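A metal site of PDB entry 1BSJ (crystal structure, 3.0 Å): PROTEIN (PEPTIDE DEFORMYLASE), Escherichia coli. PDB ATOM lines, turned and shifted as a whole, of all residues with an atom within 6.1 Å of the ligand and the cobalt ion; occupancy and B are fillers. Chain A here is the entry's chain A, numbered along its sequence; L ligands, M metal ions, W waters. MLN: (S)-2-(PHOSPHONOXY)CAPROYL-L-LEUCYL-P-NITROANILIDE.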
ATOM      1  N   GLU A  41      18.934  12.889  29.193  1.00  0.00           N
ATOM      2  CA  GLU A  41      18.577  11.692  28.433  1.00  0.00           C
ATOM      3  C   GLU A  41      19.756  10.745  28.263  1.00  0.00           C
ATOM      4  O   GLU A  41      19.635   9.732  27.609  1.00  0.00           O
ATOM      5  CB  GLU A  41      18.089  12.077  27.054  1.00  0.00           C
ATOM      6  CG  GLU A  41      17.070  13.199  27.032  1.00  0.00           C
ATOM      7  CD  GLU A  41      15.655  12.716  27.237  1.00  0.00           C
ATOM      8  OE1 GLU A  41      15.351  12.281  28.360  1.00  0.00           O
ATOM      9  OE2 GLU A  41      14.838  12.790  26.282  1.00  0.00           O
ATOM     10  N   GLU A  42      20.918  11.101  28.805  1.00  0.00           N
ATOM     11  CA  GLU A  42      22.104  10.261  28.709  1.00  0.00           C
ATOM     12  C   GLU A  42      22.637  10.107  27.266  1.00  0.00           C
ATOM     13  O   GLU A  42      23.190   9.058  26.899  1.00  0.00           O
ATOM     14  CB  GLU A  42      21.872   8.886  29.341  1.00  0.00           C
ATOM     15  CG  GLU A  42      21.526   8.941  30.816  1.00  0.00           C
ATOM     16  CD  GLU A  42      21.550   7.577  31.482  1.00  0.00           C
ATOM     17  OE1 GLU A  42      20.538   6.852  31.394  1.00  0.00           O
ATOM     18  OE2 GLU A  42      22.583   7.214  32.089  1.00  0.00           O
ATOM     19  N   GLY A  43      22.480  11.158  26.468  1.00  0.00           N
ATOM     20  CA  GLY A  43      22.948  11.142  25.096  1.00  0.00           C
ATOM     21  C   GLY A  43      24.348  11.698  25.042  1.00  0.00           C
ATOM     22  O   GLY A  43      24.758  12.352  25.998  1.00  0.00           O
ATOM     23  N   ILE A  44      25.082  11.430  23.956  1.00  0.00           N
ATOM     24  CA  ILE A  44      26.439  11.944  23.832  1.00  0.00           C
ATOM     25  C   ILE A  44      26.528  13.137  22.886  1.00  0.00           C
ATOM     26  O   ILE A  44      27.602  13.688  22.667  1.00  0.00           O
ATOM     27  CB  ILE A  44      27.452  10.846  23.408  1.00  0.00           C
ATOM     28  CG1 ILE A  44      27.195  10.393  21.967  1.00  0.00           C
ATOM     29  CG2 ILE A  44      27.332   9.643  24.322  1.00  0.00           C
ATOM     30  CD1 ILE A  44      28.084   9.201  21.510  1.00  0.00           C
ATOM     31  N   GLY A  45      25.386  13.553  22.352  1.00  0.00           N
ATOM     32  CA  GLY A  45      25.315  14.675  21.449  1.00  0.00           C
ATOM     33  C   GLY A  45      23.861  15.077  21.266  1.00  0.00           C
ATOM     34  O   GLY A  45      22.977  14.310  21.629  1.00  0.00           O
ATOM     35  N   LEU A  46      23.606  16.272  20.734  1.00  0.00           N
ATOM     36  CA  LEU A  46      22.230  16.745  20.527  1.00  0.00           C
ATOM     37  C   LEU A  46      22.218  17.921  19.550  1.00  0.00           C
ATOM     38  O   LEU A  46      22.896  18.942  19.775  1.00  0.00           O
ATOM     39  CB  LEU A  46      21.583  17.212  21.838  1.00  0.00           C
ATOM     40  CG  LEU A  46      20.097  17.590  21.773  1.00  0.00           C
ATOM     41  CD1 LEU A  46      19.247  16.333  21.715  1.00  0.00           C
ATOM     42  CD2 LEU A  46      19.694  18.409  22.960  1.00  0.00           C
ATOM     43  N   ALA A  47      21.470  17.770  18.471  1.00  0.00           N
ATOM     44  CA  ALA A  47      21.353  18.802  17.470  1.00  0.00           C
ATOM     45  C   ALA A  47      20.092  19.606  17.767  1.00  0.00           C
ATOM     46  O   ALA A  47      19.103  19.047  18.217  1.00  0.00           O
ATOM     47  CB  ALA A  47      21.278  18.189  16.108  1.00  0.00           C
ATOM     48  N   GLN A  50      16.431  18.548  16.829  1.00  0.00           N
ATOM     49  CA  GLN A  50      15.752  17.513  17.606  1.00  0.00           C
ATOM     50  C   GLN A  50      14.837  18.108  18.662  1.00  0.00           C
ATOM     51  O   GLN A  50      13.899  17.455  19.114  1.00  0.00           O
ATOM     52  CB  GLN A  50      16.767  16.611  18.296  1.00  0.00           C
ATOM     53  CG  GLN A  50      17.623  15.787  17.362  1.00  0.00           C
ATOM     54  CD  GLN A  50      18.670  14.992  18.126  1.00  0.00           C
ATOM     55  OE1 GLN A  50      19.805  15.432  18.267  1.00  0.00           O
ATOM     56  NE2 GLN A  50      18.288  13.844  18.640  1.00  0.00           N
ATOM     57  N   ILE A  86      29.651   2.264  13.930  1.00  0.00           N
ATOM     58  CA  ILE A  86      29.244   1.746  15.226  1.00  0.00           C
ATOM     59  C   ILE A  86      27.716   1.600  15.243  1.00  0.00           C
ATOM     60  O   ILE A  86      27.027   2.059  14.322  1.00  0.00           O
ATOM     61  CB  ILE A  86      29.647   2.687  16.391  1.00  0.00           C
ATOM     62  CG1 ILE A  86      28.874   4.005  16.320  1.00  0.00           C
ATOM     63  CG2 ILE A  86      31.126   2.982  16.379  1.00  0.00           C
ATOM     64  CD1 ILE A  86      29.045   4.826  17.560  1.00  0.00           C
ATOM     65  N   GLU A  87      27.185   0.918  16.256  1.00  0.00           N
ATOM     66  CA  GLU A  87      25.756   0.746  16.392  1.00  0.00           C
ATOM     67  C   GLU A  87      25.203   2.040  16.960  1.00  0.00           C
ATOM     68  O   GLU A  87      25.084   2.202  18.179  1.00  0.00           O
ATOM     69  CB  GLU A  87      25.435  -0.379  17.365  1.00  0.00           C
ATOM     70  CG  GLU A  87      26.231  -1.623  17.136  1.00  0.00           C
ATOM     71  CD  GLU A  87      25.432  -2.700  16.446  1.00  0.00           C
ATOM     72  OE1 GLU A  87      24.953  -2.429  15.325  1.00  0.00           O
ATOM     73  OE2 GLU A  87      25.289  -3.796  17.025  1.00  0.00           O
ATOM     74  N   GLU A  88      24.867   2.961  16.076  1.00  0.00           N
ATOM     75  CA  GLU A  88      24.338   4.252  16.511  1.00  0.00           C
ATOM     76  C   GLU A  88      22.909   4.165  16.973  1.00  0.00           C
ATOM     77  O   GLU A  88      22.155   3.275  16.575  1.00  0.00           O
ATOM     78  CB  GLU A  88      24.444   5.268  15.377  1.00  0.00           C
ATOM     79  CG  GLU A  88      25.851   5.589  15.002  1.00  0.00           C
ATOM     80  CD  GLU A  88      25.956   6.590  13.885  1.00  0.00           C
ATOM     81  OE1 GLU A  88      25.116   7.517  13.841  1.00  0.00           O
ATOM     82  OE2 GLU A  88      26.888   6.457  13.066  1.00  0.00           O
ATOM     83  N   GLY A  89      22.557   5.103  17.831  1.00  0.00           N
ATOM     84  CA  GLY A  89      21.215   5.199  18.366  1.00  0.00           C
ATOM     85  C   GLY A  89      20.891   6.665  18.265  1.00  0.00           C
ATOM     86  O   GLY A  89      21.727   7.447  17.824  1.00  0.00           O
ATOM     87  N   CYS A  90      19.668   7.045  18.605  1.00  0.00           N
ATOM     88  CA  CYS A  90      19.268   8.428  18.493  1.00  0.00           C
ATOM     89  C   CYS A  90      18.070   8.642  19.436  1.00  0.00           C
ATOM     90  O   CYS A  90      17.209   7.775  19.549  1.00  0.00           O
ATOM     91  CB  CYS A  90      18.907   8.682  17.029  1.00  0.00           C
ATOM     92  SG  CYS A  90      18.456  10.410  16.716  1.00  0.00           S
ATOM     93  N   LEU A  91      18.002   9.781  20.095  1.00  0.00           N
ATOM     94  CA  LEU A  91      16.897  10.039  21.001  1.00  0.00           C
ATOM     95  C   LEU A  91      15.585  10.175  20.218  1.00  0.00           C
ATOM     96  O   LEU A  91      14.513   9.888  20.756  1.00  0.00           O
ATOM     97  CB  LEU A  91      17.189  11.279  21.848  1.00  0.00           C
ATOM     98  CG  LEU A  91      18.308  11.048  22.884  1.00  0.00           C
ATOM     99  CD1 LEU A  91      18.787  12.372  23.447  1.00  0.00           C
ATOM    100  CD2 LEU A  91      17.849  10.107  24.002  1.00  0.00           C
ATOM    101  N   SER A  92      15.708  10.544  18.933  1.00  0.00           N
ATOM    102  CA  SER A  92      14.563  10.735  18.043  1.00  0.00           C
ATOM    103  C   SER A  92      14.074   9.447  17.390  1.00  0.00           C
ATOM    104  O   SER A  92      13.073   9.443  16.667  1.00  0.00           O
ATOM    105  CB  SER A  92      14.884  11.776  16.971  1.00  0.00           C
ATOM    106  OG  SER A  92      15.152  13.040  17.551  1.00  0.00           O
ATOM    107  N   ARG A  97      18.870   0.649  16.840  1.00  0.00           N
ATOM    108  CA  ARG A  97      20.296   0.845  16.682  1.00  0.00           C
ATOM    109  C   ARG A  97      20.724   0.198  15.389  1.00  0.00           C
ATOM    110  O   ARG A  97      20.295  -0.893  15.069  1.00  0.00           O
ATOM    111  CB  ARG A  97      21.059   0.173  17.828  1.00  0.00           C
ATOM    112  CG  ARG A  97      20.716   0.676  19.213  1.00  0.00           C
ATOM    113  CD  ARG A  97      21.857   1.430  19.833  1.00  0.00           C
ATOM    114  NE  ARG A  97      21.447   2.037  21.095  1.00  0.00           N
ATOM    115  CZ  ARG A  97      22.274   2.262  22.116  1.00  0.00           C
ATOM    116  NH1 ARG A  97      23.561   1.937  22.034  1.00  0.00           N
ATOM    117  NH2 ARG A  97      21.794   2.781  23.262  1.00  0.00           N
ATOM    118  N   LEU A 125      35.146   8.070  18.238  1.00  0.00           N
ATOM    119  CA  LEU A 125      33.762   8.337  18.541  1.00  0.00           C
ATOM    120  C   LEU A 125      33.355   9.787  18.306  1.00  0.00           C
ATOM    121  O   LEU A 125      32.266  10.060  17.774  1.00  0.00           O
ATOM    122  CB  LEU A 125      33.465   7.946  19.982  1.00  0.00           C
ATOM    123  CG  LEU A 125      32.005   7.942  20.397  1.00  0.00           C
ATOM    124  CD1 LEU A 125      31.302   6.781  19.747  1.00  0.00           C
ATOM    125  CD2 LEU A 125      31.888   7.845  21.914  1.00  0.00           C
ATOM    126  N   ILE A 128      32.541  10.404  14.720  1.00  0.00           N
ATOM    127  CA  ILE A 128      31.263   9.823  14.362  1.00  0.00           C
ATOM    128  C   ILE A 128      30.095  10.671  14.849  1.00  0.00           C
ATOM    129  O   ILE A 128      29.194  11.003  14.072  1.00  0.00           O
ATOM    130  CB  ILE A 128      31.123   8.394  14.931  1.00  0.00           C
ATOM    131  CG1 ILE A 128      32.226   7.505  14.355  1.00  0.00           C
ATOM    132  CG2 ILE A 128      29.754   7.827  14.597  1.00  0.00           C
ATOM    133  CD1 ILE A 128      32.120   6.088  14.771  1.00  0.00           C
ATOM    134  N   CYS A 129      30.156  11.059  16.121  1.00  0.00           N
ATOM    135  CA  CYS A 129      29.122  11.871  16.746  1.00  0.00           C
ATOM    136  C   CYS A 129      28.894  13.131  15.938  1.00  0.00           C
ATOM    137  O   CYS A 129      27.762  13.432  15.586  1.00  0.00           O
ATOM    138  CB  CYS A 129      29.533  12.208  18.164  1.00  0.00           C
ATOM    139  SG  CYS A 129      28.263  12.954  19.146  1.00  0.00           S
ATOM    140  N   HIS A 132      26.971  12.499  12.865  1.00  0.00           N
ATOM    141  CA  HIS A 132      25.587  12.200  13.220  1.00  0.00           C
ATOM    142  C   HIS A 132      24.835  13.490  13.485  1.00  0.00           C
ATOM    143  O   HIS A 132      23.765  13.714  12.928  1.00  0.00           O
ATOM    144  CB  HIS A 132      25.548  11.295  14.449  1.00  0.00           C
ATOM    145  CG  HIS A 132      24.160  10.911  14.889  1.00  0.00           C
ATOM    146  ND1 HIS A 132      23.680   9.636  14.916  1.00  0.00           N
ATOM    147  CD2 HIS A 132      23.174  11.678  15.438  1.00  0.00           C
ATOM    148  CE1 HIS A 132      22.468   9.634  15.486  1.00  0.00           C
ATOM    149  NE2 HIS A 132      22.144  10.865  15.813  1.00  0.00           N
ATOM    150  N   GLU A 133      25.377  14.301  14.375  1.00  0.00           N
ATOM    151  CA  GLU A 133      24.769  15.570  14.757  1.00  0.00           C
ATOM    152  C   GLU A 133      24.616  16.558  13.622  1.00  0.00           C
ATOM    153  O   GLU A 133      23.644  17.297  13.584  1.00  0.00           O
ATOM    154  CB  GLU A 133      25.553  16.212  15.897  1.00  0.00           C
ATOM    155  CG  GLU A 133      25.563  15.374  17.151  1.00  0.00           C
ATOM    156  CD  GLU A 133      24.195  14.859  17.541  1.00  0.00           C
ATOM    157  OE1 GLU A 133      23.183  15.588  17.384  1.00  0.00           O
ATOM    158  OE2 GLU A 133      24.119  13.720  18.017  1.00  0.00           O
ATOM    159  N   HIS A 136      21.726  15.730  11.392  1.00  0.00           N
ATOM    160  CA  HIS A 136      20.505  16.213  12.025  1.00  0.00           C
ATOM    161  C   HIS A 136      20.179  17.643  11.596  1.00  0.00           C
ATOM    162  O   HIS A 136      19.007  18.005  11.543  1.00  0.00           O
ATOM    163  CB  HIS A 136      20.649  16.215  13.549  1.00  0.00           C
ATOM    164  CG  HIS A 136      20.131  14.981  14.198  1.00  0.00           C
ATOM    165  ND1 HIS A 136      18.905  14.419  13.926  1.00  0.00           N
ATOM    166  CD2 HIS A 136      20.710  14.171  15.118  1.00  0.00           C
ATOM    167  CE1 HIS A 136      18.795  13.310  14.651  1.00  0.00           C
ATOM    168  NE2 HIS A 136      19.868  13.134  15.386  1.00  0.00           N
ATOM    169  N   LEU A 141      18.511  11.713   9.131  1.00  0.00           N
ATOM    170  CA  LEU A 141      18.533  10.825  10.307  1.00  0.00           C
ATOM    171  C   LEU A 141      19.392   9.625   9.952  1.00  0.00           C
ATOM    172  O   LEU A 141      19.534   9.325   8.763  1.00  0.00           O
ATOM    173  CB  LEU A 141      17.121  10.359  10.629  1.00  0.00           C
ATOM    174  CG  LEU A 141      16.217  11.488  11.155  1.00  0.00           C
ATOM    175  CD1 LEU A 141      14.773  11.073  11.067  1.00  0.00           C
ATOM    176  CD2 LEU A 141      16.585  11.784  12.578  1.00  0.00           C
ATOM    177  N   PHE A 142      19.909   8.916  10.946  1.00  0.00           N
ATOM    178  CA  PHE A 142      20.754   7.764  10.629  1.00  0.00           C
ATOM    179  C   PHE A 142      20.079   6.618   9.871  1.00  0.00           C
ATOM    180  O   PHE A 142      20.758   5.823   9.243  1.00  0.00           O
ATOM    181  CB  PHE A 142      21.491   7.241  11.872  1.00  0.00           C
ATOM    182  CG  PHE A 142      20.679   6.315  12.744  1.00  0.00           C
ATOM    183  CD1 PHE A 142      20.435   4.999  12.353  1.00  0.00           C
ATOM    184  CD2 PHE A 142      20.173   6.753  13.939  1.00  0.00           C
ATOM    185  CE1 PHE A 142      19.697   4.140  13.176  1.00  0.00           C
ATOM    186  CE2 PHE A 142      19.435   5.907  14.764  1.00  0.00           C
ATOM    187  CZ  PHE A 142      19.195   4.598  14.379  1.00  0.00           C
HETATM  188  O3  MLN L   1      21.448  12.806  18.340  1.00  0.00           O
HETATM  189  P1  MLN L   1      21.257  12.398  19.856  1.00  0.00           P
HETATM  190  O2  MLN L   1      22.678  11.542  20.214  1.00  0.00           O
HETATM  191  O4  MLN L   1      20.100  11.372  19.845  1.00  0.00           O
HETATM  192  C5  MLN L   1      22.875  10.303  19.606  1.00  0.00           C
HETATM  193  C6  MLN L   1      23.155   9.512  20.898  1.00  0.00           C
HETATM  194  C7  MLN L   1      24.102  10.609  18.714  1.00  0.00           C
HETATM  195  C8  MLN L   1      25.427  10.043  19.120  1.00  0.00           C
HETATM  196  C9  MLN L   1      26.319   9.423  18.026  1.00  0.00           C
HETATM  197  C10 MLN L   1      25.518   8.226  17.575  1.00  0.00           C
HETATM  198  O11 MLN L   1      23.534  10.076  21.915  1.00  0.00           O
HETATM  199  N12 MLN L   1      22.932   8.154  20.824  1.00  0.00           N
HETATM  200  C13 MLN L   1      23.244   7.208  21.914  1.00  0.00           C
HETATM  201  C14 MLN L   1      21.989   6.462  22.402  1.00  0.00           C
HETATM  202  C15 MLN L   1      20.981   7.490  22.907  1.00  0.00           C
HETATM  203  C16 MLN L   1      19.598   6.945  22.894  1.00  0.00           C
HETATM  204  C17 MLN L   1      21.030   7.928  24.334  1.00  0.00           C
HETATM  205  C18 MLN L   1      24.317   6.286  21.328  1.00  0.00           C
HETATM  206  N19 MLN L   1      25.608   6.142  22.114  1.00  0.00           N
HETATM  207  O20 MLN L   1      24.190   5.661  20.281  1.00  0.00           O
HETATM  208  C21 MLN L   1      26.620   5.367  21.891  1.00  0.00           C
HETATM  209  C22 MLN L   1      26.582   4.389  20.879  1.00  0.00           C
HETATM  210  C23 MLN L   1      27.699   3.558  20.710  1.00  0.00           C
HETATM  211  C24 MLN L   1      28.853   3.769  21.535  1.00  0.00           C
HETATM  212  C25 MLN L   1      28.911   4.768  22.544  1.00  0.00           C
HETATM  213  C26 MLN L   1      27.759   5.571  22.732  1.00  0.00           C
HETATM  214  N27 MLN L   1      29.988   2.939  21.338  1.00  0.00           N
HETATM  215  O28 MLN L   1      31.066   3.231  22.084  1.00  0.00           O
HETATM  216  O29 MLN L   1      29.999   1.921  20.458  1.00  0.00           O
HETATM  217 CO    CO M   1      20.474  11.674  16.759  1.00  0.00          CO
HETATM  218  O   HOH W   1      19.872  10.290  13.850  1.00  0.00           O
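The backbone carbonyl oxygen of Gly 45 lies close to an oxygen (O2) of the ligand (3.1 Å).
Glu 41 touches the ligand.
Glu 42 touches the ligand (O to C17, 3.5 Å).
Gly 43 touches the ligand (CA to O11, 3.4 Å).
Ile 86 touches the ligand (CD1 to C23, 3.7 Å).
Glu 87 touches the ligand (O to C22, 3.8 Å).
CG of Glu 88 touches C10 of the ligand, at 3.7 Å.
Arg 97 touches the ligand (NH2 to C14, 3.8 Å).
Cys 129 touches the ligand.
Hydrophobic or aromatic side chains within 4 Å of the ligand: Ile 44, Ile 86, Leu 91, His 132 and His 136.
17 residues have an atom within 4 Å of the ligand: Glu 41, Glu 42, Gly 43, Ile 44, Gly 45, Gln 50, Ile 86, Glu 87, Glu 88, Gly 89, Cys 90, Leu 91, Arg 97, Cys 129, His 132, Glu 133 and His 136.
Along chain A the residues within 4 Å of the ligand span positions 41 to 136.
The nearest printed residue that does not touch the ligand is Leu 125 (4.2 Å).
OE1 of Glu 133 lies close to OE1 of Gln 50.
The side-chain sulfur (SG) of Cys 90 sits close to the backbone NH (N) of Ser 92 (3.5 Å).
The side-chain amide oxygen of Gln 50 is in hydrogen-bond range of the backbone NH of Ala 47, at 2.9 Å.
O of Ile 44 sits at hydrogen-bond distance from SG of Cys 129.
The side-chain carboxylate of Glu 133 sits close to the backbone NH of Leu 46.
The side-chain amide nitrogen (NE2) of Gln 50 lies within hydrogen-bond range of the side-chain hydroxyl (OG) of Ser 92, at 3.4 Å.
N of Ala 47 is in hydrogen-bond range of OE1 of Glu 133, at 3.0 Å.
A ring nitrogen (ND1) of His 132 is in hydrogen-bond range of the side-chain carboxylate of Glu 88.
O of Gly 89 sits at hydrogen-bond distance from N12 of the ligand, at 3.3 Å.
The side-chain amide nitrogen (NE2) of Gln 50 is in hydrogen-bond range of an oxygen (O4) of the ligand (3.3 Å).
The backbone NH of Gly 89 lies within hydrogen-bond range of an oxygen (O20) of the ligand, 3.0 Å away.
An oxygen (O4) of the ligand sits at hydrogen-bond distance from the backbone NH of Leu 91.
N of Ile 44 lies within hydrogen-bond range of O11 of the ligand.
OE2 of Glu 133 sits close to O3 of the ligand, at 2.8 Å.
NE2 of Gln 50 touches the cobalt ion, 3.6 Å away.
Along chain A the residues within 4 Å of the cobalt ion span positions 50 to 136.
The cobalt ion is bound by NE2 of His 132, NE2 of His 136, O3 of the ligand and SG of Cys 90.
The cobalt ion has four donor atoms within binding distance.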
